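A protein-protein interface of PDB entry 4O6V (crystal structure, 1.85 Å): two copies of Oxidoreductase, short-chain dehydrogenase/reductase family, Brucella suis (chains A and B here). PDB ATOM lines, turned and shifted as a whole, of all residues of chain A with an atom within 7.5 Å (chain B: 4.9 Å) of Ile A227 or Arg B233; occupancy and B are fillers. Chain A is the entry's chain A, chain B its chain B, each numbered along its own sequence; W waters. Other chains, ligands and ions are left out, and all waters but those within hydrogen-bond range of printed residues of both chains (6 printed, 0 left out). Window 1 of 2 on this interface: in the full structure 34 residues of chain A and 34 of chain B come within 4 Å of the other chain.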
ATOM      1  N   VAL A 136      -6.227  16.279 -12.200  1.00  0.00           N
ATOM      2  CA  VAL A 136      -5.373  17.149 -13.057  1.00  0.00           C
ATOM      3  C   VAL A 136      -6.230  18.246 -13.699  1.00  0.00           C
ATOM      4  O   VAL A 136      -7.298  17.956 -14.232  1.00  0.00           O
ATOM      5  CB  VAL A 136      -4.763  16.320 -14.186  1.00  0.00           C
ATOM      6  CG1 VAL A 136      -4.262  17.172 -15.323  1.00  0.00           C
ATOM      7  CG2 VAL A 136      -3.672  15.411 -13.619  1.00  0.00           C
ATOM      8  N   LYS A 167      -0.077  28.603  -9.356  1.00  0.00           N
ATOM      9  CA  LYS A 167       0.945  28.238  -8.375  1.00  0.00           C
ATOM     10  C   LYS A 167       0.321  28.152  -6.962  1.00  0.00           C
ATOM     11  O   LYS A 167       0.570  27.201  -6.224  1.00  0.00           O
ATOM     12  CB  LYS A 167       2.097  29.230  -8.411  1.00  0.00           C
ATOM     13  CG  LYS A 167       3.200  28.971  -7.409  1.00  0.00           C
ATOM     14  CD  LYS A 167       3.704  27.544  -7.574  1.00  0.00           C
ATOM     15  CE  LYS A 167       4.973  27.301  -6.822  1.00  0.00           C
ATOM     16  NZ  LYS A 167       5.366  25.888  -7.026  1.00  0.00           N
ATOM     17  N   ALA A 170      -1.718  24.946  -6.936  1.00  0.00           N
ATOM     18  CA  ALA A 170      -0.819  23.788  -6.903  1.00  0.00           C
ATOM     19  C   ALA A 170      -0.264  23.563  -5.503  1.00  0.00           C
ATOM     20  O   ALA A 170      -0.196  22.397  -5.010  1.00  0.00           O
ATOM     21  CB  ALA A 170       0.328  23.980  -7.885  1.00  0.00           C
ATOM     22  N   ILE A 178      -3.630  16.530  -6.331  1.00  0.00           N
ATOM     23  CA  ILE A 178      -4.357  17.264  -7.347  1.00  0.00           C
ATOM     24  C   ILE A 178      -3.402  18.321  -7.923  1.00  0.00           C
ATOM     25  O   ILE A 178      -2.843  19.162  -7.166  1.00  0.00           O
ATOM     26  CB  ILE A 178      -5.621  17.937  -6.763  1.00  0.00           C
ATOM     27  CG1 ILE A 178      -6.508  16.880  -6.095  1.00  0.00           C
ATOM     28  CG2 ILE A 178      -6.315  18.745  -7.864  1.00  0.00           C
ATOM     29  CD1 ILE A 178      -7.689  17.436  -5.330  1.00  0.00           C
ATOM     30  N   ARG A 179      -3.171  18.238  -9.240  1.00  0.00           N
ATOM     31  CA  ARG A 179      -2.179  19.069  -9.932  1.00  0.00           C
ATOM     32  C   ARG A 179      -2.856  20.026 -10.926  1.00  0.00           C
ATOM     33  O   ARG A 179      -3.928  19.744 -11.460  1.00  0.00           O
ATOM     34  CB  ARG A 179      -1.143  18.168 -10.673  1.00  0.00           C
ATOM     35  CG  ARG A 179      -0.347  17.189  -9.807  1.00  0.00           C
ATOM     36  CD  ARG A 179      -1.003  15.828  -9.635  1.00  0.00           C
ATOM     37  NE  ARG A 179      -0.994  15.029 -10.864  1.00  0.00           N
ATOM     38  CZ  ARG A 179      -1.590  13.874 -11.011  1.00  0.00           C
ATOM     39  NH1 ARG A 179      -2.302  13.336 -10.010  1.00  0.00           N
ATOM     40  NH2 ARG A 179      -1.471  13.215 -12.175  1.00  0.00           N
ATOM     41  N   MET A 180      -2.247  21.188 -11.117  1.00  0.00           N
ATOM     42  CA  MET A 180      -2.636  22.149 -12.147  1.00  0.00           C
ATOM     43  C   MET A 180      -1.421  22.650 -12.899  1.00  0.00           C
ATOM     44  O   MET A 180      -0.427  23.013 -12.285  1.00  0.00           O
ATOM     45  CB  MET A 180      -3.394  23.329 -11.550  1.00  0.00           C
ATOM     46  CG  MET A 180      -4.039  24.246 -12.593  1.00  0.00           C
ATOM     47  SD  MET A 180      -4.882  25.680 -11.874  1.00  0.00           S
ATOM     48  CE  MET A 180      -6.363  24.886 -11.197  1.00  0.00           C
ATOM     49  N   ASN A 181      -1.501  22.621 -14.226  1.00  0.00           N
ATOM     50  CA  ASN A 181      -0.472  23.147 -15.110  1.00  0.00           C
ATOM     51  C   ASN A 181      -1.111  23.873 -16.292  1.00  0.00           C
ATOM     52  O   ASN A 181      -2.265  23.608 -16.652  1.00  0.00           O
ATOM     53  CB  ASN A 181       0.420  22.021 -15.664  1.00  0.00           C
ATOM     54  CG  ASN A 181       1.204  21.322 -14.596  1.00  0.00           C
ATOM     55  OD1 ASN A 181       2.139  21.894 -13.992  1.00  0.00           O
ATOM     56  ND2 ASN A 181       0.829  20.062 -14.315  1.00  0.00           N
ATOM     57  N   PHE A 218      -0.130  14.389 -22.523  1.00  0.00           N
ATOM     58  CA  PHE A 218       0.992  14.037 -21.626  1.00  0.00           C
ATOM     59  C   PHE A 218       0.690  14.513 -20.189  1.00  0.00           C
ATOM     60  O   PHE A 218       0.815  13.747 -19.211  1.00  0.00           O
ATOM     61  CB  PHE A 218       2.307  14.629 -22.111  1.00  0.00           C
ATOM     62  CG  PHE A 218       3.397  14.540 -21.074  1.00  0.00           C
ATOM     63  CD1 PHE A 218       3.876  13.304 -20.690  1.00  0.00           C
ATOM     64  CD2 PHE A 218       3.937  15.679 -20.495  1.00  0.00           C
ATOM     65  CE1 PHE A 218       4.868  13.215 -19.695  1.00  0.00           C
ATOM     66  CE2 PHE A 218       4.936  15.592 -19.533  1.00  0.00           C
ATOM     67  CZ  PHE A 218       5.397  14.361 -19.128  1.00  0.00           C
ATOM     68  N   LEU A 219       0.262  15.760 -20.054  1.00  0.00           N
ATOM     69  CA  LEU A 219      -0.019  16.312 -18.735  1.00  0.00           C
ATOM     70  C   LEU A 219      -1.199  15.626 -18.030  1.00  0.00           C
ATOM     71  O   LEU A 219      -1.268  15.671 -16.811  1.00  0.00           O
ATOM     72  CB  LEU A 219      -0.206  17.832 -18.823  1.00  0.00           C
ATOM     73  CG  LEU A 219       1.048  18.639 -19.188  1.00  0.00           C
ATOM     74  CD1 LEU A 219       0.702  20.086 -19.474  1.00  0.00           C
ATOM     75  CD2 LEU A 219       2.147  18.536 -18.149  1.00  0.00           C
ATOM     76  N   ASP A 222      -0.360   9.517 -16.205  1.00  0.00           N
ATOM     77  CA  ASP A 222       0.375   9.196 -14.962  1.00  0.00           C
ATOM     78  C   ASP A 222       1.868   9.538 -15.020  1.00  0.00           C
ATOM     79  O   ASP A 222       2.481   9.878 -13.987  1.00  0.00           O
ATOM     80  CB  ASP A 222       0.225   7.703 -14.607  1.00  0.00           C
ATOM     81  CG  ASP A 222      -1.165   7.338 -14.143  1.00  0.00           C
ATOM     82  OD1 ASP A 222      -2.024   8.210 -13.885  1.00  0.00           O
ATOM     83  OD2 ASP A 222      -1.375   6.109 -14.014  1.00  0.00           O
ATOM     84  N   GLY A 223       2.451   9.514 -16.206  1.00  0.00           N
ATOM     85  CA  GLY A 223       3.878   9.818 -16.353  1.00  0.00           C
ATOM     86  C   GLY A 223       4.247  11.249 -15.940  1.00  0.00           C
ATOM     87  O   GLY A 223       5.385  11.510 -15.496  1.00  0.00           O
ATOM     88  N   ALA A 224       3.279  12.162 -16.093  1.00  0.00           N
ATOM     89  CA  ALA A 224       3.453  13.562 -15.746  1.00  0.00           C
ATOM     90  C   ALA A 224       3.046  13.889 -14.289  1.00  0.00           C
ATOM     91  O   ALA A 224       2.966  15.072 -13.960  1.00  0.00           O
ATOM     92  CB  ALA A 224       2.634  14.409 -16.712  1.00  0.00           C
ATOM     93  N   ALA A 225       2.786  12.882 -13.428  1.00  0.00           N
ATOM     94  CA  ALA A 225       2.119  13.129 -12.126  1.00  0.00           C
ATOM     95  C   ALA A 225       2.975  14.001 -11.189  1.00  0.00           C
ATOM     96  O   ALA A 225       2.413  14.651 -10.289  1.00  0.00           O
ATOM     97  CB  ALA A 225       1.743  11.838 -11.413  1.00  0.00           C
ATOM     98  N   TYR A 226       4.306  14.034 -11.387  1.00  0.00           N
ATOM     99  CA  TYR A 226       5.137  14.868 -10.499  1.00  0.00           C
ATOM    100  C   TYR A 226       5.285  16.290 -11.019  1.00  0.00           C
ATOM    101  O   TYR A 226       6.006  17.056 -10.406  1.00  0.00           O
ATOM    102  CB  TYR A 226       6.502  14.264 -10.296  1.00  0.00           C
ATOM    103  CG  TYR A 226       7.211  14.604  -8.969  1.00  0.00           C
ATOM    104  CD1 TYR A 226       6.583  14.427  -7.731  1.00  0.00           C
ATOM    105  CD2 TYR A 226       8.523  15.038  -8.978  1.00  0.00           C
ATOM    106  CE1 TYR A 226       7.263  14.680  -6.535  1.00  0.00           C
ATOM    107  CE2 TYR A 226       9.209  15.301  -7.813  1.00  0.00           C
ATOM    108  CZ  TYR A 226       8.557  15.122  -6.568  1.00  0.00           C
ATOM    109  OH  TYR A 226       9.251  15.354  -5.385  1.00  0.00           O
ATOM    110  N   ILE A 227       4.595  16.653 -12.100  1.00  0.00           N
ATOM    111  CA  ILE A 227       4.589  18.060 -12.584  1.00  0.00           C
ATOM    112  C   ILE A 227       3.385  18.828 -12.052  1.00  0.00           C
ATOM    113  O   ILE A 227       2.258  18.411 -12.261  1.00  0.00           O
ATOM    114  CB  ILE A 227       4.580  18.122 -14.120  1.00  0.00           C
ATOM    115  CG1 ILE A 227       5.724  17.297 -14.652  1.00  0.00           C
ATOM    116  CG2 ILE A 227       4.686  19.561 -14.609  1.00  0.00           C
ATOM    117  CD1 ILE A 227       5.734  17.092 -16.150  1.00  0.00           C
ATOM    118  N   THR A 228       3.623  19.956 -11.373  1.00  0.00           N
ATOM    119  CA  THR A 228       2.526  20.806 -10.930  1.00  0.00           C
ATOM    120  C   THR A 228       3.005  22.267 -10.779  1.00  0.00           C
ATOM    121  O   THR A 228       4.191  22.511 -10.479  1.00  0.00           O
ATOM    122  CB  THR A 228       1.861  20.263  -9.647  1.00  0.00           C
ATOM    123  OG1 THR A 228       0.606  20.915  -9.465  1.00  0.00           O
ATOM    124  CG2 THR A 228       2.745  20.474  -8.392  1.00  0.00           C
ATOM    125  N   GLY A 229       2.087  23.180 -11.061  1.00  0.00           N
ATOM    126  CA  GLY A 229       2.322  24.602 -10.963  1.00  0.00           C
ATOM    127  C   GLY A 229       3.053  25.186 -12.157  1.00  0.00           C
ATOM    128  O   GLY A 229       3.445  26.338 -12.092  1.00  0.00           O
ATOM    129  N   GLN A 230       3.272  24.403 -13.220  1.00  0.00           N
ATOM    130  CA  GLN A 230       4.107  24.826 -14.348  1.00  0.00           C
ATOM    131  C   GLN A 230       3.391  25.504 -15.517  1.00  0.00           C
ATOM    132  O   GLN A 230       2.175  25.365 -15.701  1.00  0.00           O
ATOM    133  CB  GLN A 230       4.911  23.633 -14.877  1.00  0.00           C
ATOM    134  CG  GLN A 230       5.812  22.970 -13.814  1.00  0.00           C
ATOM    135  CD  GLN A 230       6.596  23.951 -12.980  1.00  0.00           C
ATOM    136  OE1 GLN A 230       7.342  24.786 -13.527  1.00  0.00           O
ATOM    137  NE2 GLN A 230       6.425  23.895 -11.668  1.00  0.00           N
ATOM    138  N   ASN A 231       4.186  26.293 -16.257  1.00  0.00           N
ATOM    139  CA  ASN A 231       3.786  27.011 -17.451  1.00  0.00           C
ATOM    140  C   ASN A 231       4.714  26.565 -18.589  1.00  0.00           C
ATOM    141  O   ASN A 231       5.915  26.968 -18.639  1.00  0.00           O
ATOM    142  CB  ASN A 231       3.872  28.525 -17.237  1.00  0.00           C
ATOM    143  CG  ASN A 231       2.868  29.004 -16.209  1.00  0.00           C
ATOM    144  OD1 ASN A 231       1.680  29.216 -16.518  1.00  0.00           O
ATOM    145  ND2 ASN A 231       3.317  29.109 -14.979  1.00  0.00           N
ATOM    146  N   LEU A 232       4.193  25.677 -19.435  1.00  0.00           N
ATOM    147  CA  LEU A 232       5.019  24.988 -20.478  1.00  0.00           C
ATOM    148  C   LEU A 232       4.733  25.641 -21.834  1.00  0.00           C
ATOM    149  O   LEU A 232       3.613  25.543 -22.371  1.00  0.00           O
ATOM    150  CB  LEU A 232       4.680  23.487 -20.498  1.00  0.00           C
ATOM    151  CG  LEU A 232       5.354  22.672 -21.598  1.00  0.00           C
ATOM    152  CD1 LEU A 232       6.883  22.849 -21.626  1.00  0.00           C
ATOM    153  CD2 LEU A 232       5.020  21.184 -21.386  1.00  0.00           C
ATOM    154  N   ALA B 143      16.001  21.261 -10.918  1.00  0.00           N
ATOM    155  CA  ALA B 143      14.976  22.219 -10.553  1.00  0.00           C
ATOM    156  C   ALA B 143      15.548  23.439  -9.804  1.00  0.00           C
ATOM    157  O   ALA B 143      14.883  24.461  -9.794  1.00  0.00           O
ATOM    158  CB  ALA B 143      13.869  21.584  -9.752  1.00  0.00           C
ATOM    159  N   GLU B 147      16.563  28.778  -9.036  1.00  0.00           N
ATOM    160  CA  GLU B 147      16.298  28.980  -7.610  1.00  0.00           C
ATOM    161  C   GLU B 147      17.371  28.169  -6.850  1.00  0.00           C
ATOM    162  O   GLU B 147      17.070  27.148  -6.239  1.00  0.00           O
ATOM    163  CB  GLU B 147      14.886  28.542  -7.236  1.00  0.00           C
ATOM    164  CG  GLU B 147      13.788  29.382  -7.874  1.00  0.00           C
ATOM    165  CD  GLU B 147      12.377  28.929  -7.539  1.00  0.00           C
ATOM    166  OE1 GLU B 147      12.125  28.546  -6.361  1.00  0.00           O
ATOM    167  OE2 GLU B 147      11.504  28.940  -8.472  1.00  0.00           O
ATOM    168  N   LEU B 184      14.162  19.401 -15.595  1.00  0.00           N
ATOM    169  CA  LEU B 184      14.760  19.929 -14.349  1.00  0.00           C
ATOM    170  C   LEU B 184      14.123  19.203 -13.158  1.00  0.00           C
ATOM    171  O   LEU B 184      13.099  19.635 -12.634  1.00  0.00           O
ATOM    172  CB  LEU B 184      14.511  21.455 -14.248  1.00  0.00           C
ATOM    173  CG  LEU B 184      15.461  22.349 -15.040  1.00  0.00           C
ATOM    174  CD1 LEU B 184      15.324  22.090 -16.508  1.00  0.00           C
ATOM    175  CD2 LEU B 184      15.230  23.840 -14.747  1.00  0.00           C
ATOM    176  N   THR B 215       8.875  11.903 -18.751  1.00  0.00           N
ATOM    177  CA  THR B 215       8.962  13.287 -19.268  1.00  0.00           C
ATOM    178  C   THR B 215       9.968  13.319 -20.450  1.00  0.00           C
ATOM    179  O   THR B 215       9.668  13.894 -21.508  1.00  0.00           O
ATOM    180  CB  THR B 215       9.349  14.272 -18.159  1.00  0.00           C
ATOM    181  OG1 THR B 215       8.435  14.134 -17.067  1.00  0.00           O
ATOM    182  CG2 THR B 215       9.313  15.668 -18.688  1.00  0.00           C
ATOM    183  N   ASN B 231      12.878  24.664 -20.407  1.00  0.00           N
ATOM    184  CA  ASN B 231      13.363  24.092 -19.173  1.00  0.00           C
ATOM    185  C   ASN B 231      12.166  23.698 -18.339  1.00  0.00           C
ATOM    186  O   ASN B 231      11.485  24.576 -17.794  1.00  0.00           O
ATOM    187  CB  ASN B 231      14.190  25.120 -18.409  1.00  0.00           C
ATOM    188  CG  ASN B 231      15.494  25.425 -19.125  1.00  0.00           C
ATOM    189  OD1 ASN B 231      16.483  24.668 -19.028  1.00  0.00           O
ATOM    190  ND2 ASN B 231      15.476  26.494 -19.921  1.00  0.00           N
ATOM    191  N   LEU B 232      11.875  22.402 -18.299  1.00  0.00           N
ATOM    192  CA  LEU B 232      10.663  21.900 -17.677  1.00  0.00           C
ATOM    193  C   LEU B 232      10.918  21.314 -16.300  1.00  0.00           C
ATOM    194  O   LEU B 232      11.582  20.278 -16.187  1.00  0.00           O
ATOM    195  CB  LEU B 232      10.018  20.862 -18.586  1.00  0.00           C
ATOM    196  CG  LEU B 232       8.765  20.178 -18.035  1.00  0.00           C
ATOM    197  CD1 LEU B 232       7.665  21.158 -17.608  1.00  0.00           C
ATOM    198  CD2 LEU B 232       8.246  19.233 -19.118  1.00  0.00           C
ATOM    199  N   ARG B 233      10.404  21.979 -15.264  1.00  0.00           N
ATOM    200  CA  ARG B 233      10.583  21.517 -13.872  1.00  0.00           C
ATOM    201  C   ARG B 233       9.613  20.409 -13.547  1.00  0.00           C
ATOM    202  O   ARG B 233       8.403  20.548 -13.725  1.00  0.00           O
ATOM    203  CB  ARG B 233      10.412  22.676 -12.873  1.00  0.00           C
ATOM    204  CG  ARG B 233      11.613  23.613 -12.874  1.00  0.00           C
ATOM    205  CD  ARG B 233      11.306  24.858 -12.082  1.00  0.00           C
ATOM    206  NE  ARG B 233      10.624  25.879 -12.850  1.00  0.00           N
ATOM    207  CZ  ARG B 233       9.781  26.748 -12.357  1.00  0.00           C
ATOM    208  NH1 ARG B 233       9.404  26.690 -11.071  1.00  0.00           N
ATOM    209  NH2 ARG B 233       9.306  27.688 -13.151  1.00  0.00           N
ATOM    210  N   VAL B 234      10.178  19.334 -13.011  1.00  0.00           N
ATOM    211  CA  VAL B 234       9.447  18.141 -12.605  1.00  0.00           C
ATOM    212  C   VAL B 234       9.813  17.912 -11.140  1.00  0.00           C
ATOM    213  O   VAL B 234      10.768  17.195 -10.842  1.00  0.00           O
ATOM    214  CB  VAL B 234       9.839  16.934 -13.476  1.00  0.00           C
ATOM    215  CG1 VAL B 234       8.934  15.746 -13.164  1.00  0.00           C
ATOM    216  CG2 VAL B 234       9.732  17.231 -14.979  1.00  0.00           C
ATOM    217  N   ASP B 235       9.084  18.560 -10.228  1.00  0.00           N
ATOM    218  CA  ASP B 235       9.559  18.709  -8.865  1.00  0.00           C
ATOM    219  C   ASP B 235       8.499  18.689  -7.777  1.00  0.00           C
ATOM    220  O   ASP B 235       8.772  19.132  -6.666  1.00  0.00           O
ATOM    221  CB  ASP B 235      10.378  20.017  -8.737  1.00  0.00           C
ATOM    222  CG  ASP B 235       9.524  21.299  -8.841  1.00  0.00           C
ATOM    223  OD1 ASP B 235       8.316  21.232  -9.125  1.00  0.00           O
ATOM    224  OD2 ASP B 235      10.122  22.386  -8.616  1.00  0.00           O
ATOM    225  N   THR B 239       9.816  24.144  -6.214  1.00  0.00           N
ATOM    226  CA  THR B 239      10.265  25.495  -6.521  1.00  0.00           C
ATOM    227  C   THR B 239       9.094  26.500  -6.436  1.00  0.00           C
ATOM    228  O   THR B 239       7.943  26.139  -6.604  1.00  0.00           O
ATOM    229  CB  THR B 239      10.951  25.566  -7.898  1.00  0.00           C
ATOM    230  OG1 THR B 239      10.095  25.003  -8.900  1.00  0.00           O
ATOM    231  CG2 THR B 239      12.270  24.826  -7.888  1.00  0.00           C
ATOM    232  N   SER B 241       8.757  29.721  -8.162  1.00  0.00           N
ATOM    233  CA  SER B 241       8.464  30.567  -9.286  1.00  0.00           C
ATOM    234  C   SER B 241       7.433  29.958 -10.218  1.00  0.00           C
ATOM    235  O   SER B 241       7.424  28.751 -10.470  1.00  0.00           O
ATOM    236  CB  SER B 241       9.732  30.953 -10.064  1.00  0.00           C
ATOM    237  OG  SER B 241       9.355  31.714 -11.210  1.00  0.00           O
ATOM    238  N   VAL B 242       6.529  30.814 -10.710  1.00  0.00           N
ATOM    239  CA  VAL B 242       5.666  30.411 -11.812  1.00  0.00           C
ATOM    240  C   VAL B 242       6.587  30.049 -12.987  1.00  0.00           C
ATOM    241  O   VAL B 242       7.786  30.404 -13.046  1.00  0.00           O
ATOM    242  CB  VAL B 242       4.723  31.529 -12.279  1.00  0.00           C
ATOM    243  CG1 VAL B 242       3.725  31.948 -11.185  1.00  0.00           C
ATOM    244  CG2 VAL B 242       5.515  32.742 -12.727  1.00  0.00           C
ATOM    245  OXT VAL B 242       6.105  29.473 -13.957  1.00  0.00           O
HETATM  246  O   HOH W   1       7.258  23.876  -8.696  1.00  0.00           O
HETATM  247  O   HOH W   2       5.666  26.769 -10.246  1.00  0.00           O
HETATM  248  O   HOH W   3       8.724  24.300 -15.740  1.00  0.00           O
HETATM  249  O   HOH W   4      10.935  17.638  -5.652  1.00  0.00           O
HETATM  250  O   HOH W   5       6.779  20.375 -11.355  1.00  0.00           O
HETATM  251  O   HOH W   6       6.737  27.025 -14.987  1.00  0.00           O
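The chain-end carboxylate (OXT) of Val B242 lies within hydrogen-bond range of the side-chain amide nitrogen (ND2) of Asn A231 (3.0 Å).
The backbone carbonyl oxygen (O) of Tyr A226 sits at hydrogen-bond distance from the backbone NH (N) of Asp B235 (3.4 Å).
The side-chain amino group (NZ) of Lys A167 is in hydrogen-bond range of the backbone carbonyl oxygen (O) of Thr B239.
Water W3 lies within hydrogen-bond range of the side-chain amide oxygen of Gln A230, the backbone NH of Arg B233 and the backbone carbonyl oxygen of Asn B231.
Water W2 lies within hydrogen-bond range of O of Ser B241, O of Gly A229, NE2 of Gln A230 and NZ of Lys A167.
Water W6 lies within hydrogen-bond range of OXT of Val B242 (2.7 Å), OE1 of Gln A230 (2.7 Å), N of Asn A231 (2.9 Å) and NH2 of Arg B233 (3.2 Å).
Water W4 lies within hydrogen-bond range of O of Asp B235 and OH of Tyr A226.
Water W5 lies within hydrogen-bond range of the side-chain carboxylate of Asp B235, the backbone carbonyl oxygen of Arg B233 and the backbone NH of Thr A228.
Water W1 lies within hydrogen-bond range of the side-chain carboxylate (OD1) of Asp B235 (2.9 Å), the side-chain hydroxyl (OG1) of Thr B239 (3.1 Å), the side-chain amide nitrogen (NE2) of Gln A230 (3.1 Å) and the side-chain amino group (NZ) of Lys A167 (3.2 Å).
Among the printed residues, merely in contact across the chains: Phe A218 with Thr B215 (3.7 Å), Tyr A226 with Val B234 (3.6 Å), Ile A227 with Arg B233 (3.9 Å), Ile A227 with Val B234 (3.9 Å) and Gln A230 with Arg B233 (3.3 Å).
Along chain B the printed residues that touch a printed residue of chain A span positions 215 to 242.
Hydrophobic or aromatic side chains of chain A that line the printed part of chain B: Phe A218, Tyr A226 and Ile A227.
2 positions are printed for both chains.
The side-chain amide nitrogen of Asn A181 lies within hydrogen-bond range of the backbone carbonyl oxygen of Ile A227 (3.0 Å).
NH2 of Arg B233 lies within salt-bridge range of O of Val B242.
The backbone carbonyl oxygen (O) of Thr A228 sits at hydrogen-bond distance from the side-chain amide nitrogen (NE2) of Gln A230 (2.9 Å).
The guanidinium group (NH1) of Arg B233 is in hydrogen-bond range of the side-chain hydroxyl (OG1) of Thr B239.
The side-chain hydroxyl (OG1) of Thr B239 is in hydrogen-bond range of the side-chain carboxylate (OD2) of Asp B235 (2.6 Å).
The guanidinium group (NH1) of Arg B233 sits at hydrogen-bond distance from the backbone carbonyl oxygen (O) of Ser B241 (2.9 Å).
Of the printed residues of chain B, Ile A227 touches Arg B233 (3.9 Å) and Val B234 (3.9 Å).
Of the printed residues of chain A, Thr B239 touches Lys A167.
Printed residues of chain B within 4 Å of Tyr A226: Val B234 (3.6 Å) and Asp B235 (3.4 Å).
Arg A179 touches none of the printed residues of chain B.
Asn B231 touches none of the printed residues of chain A.
The nearest printed residue of chain A that does not touch Arg B233 is Thr A228 (5.4 Å).
The nearest printed residue of chain B that does not touch Asn A231 is Ser B241 (6.1 Å).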
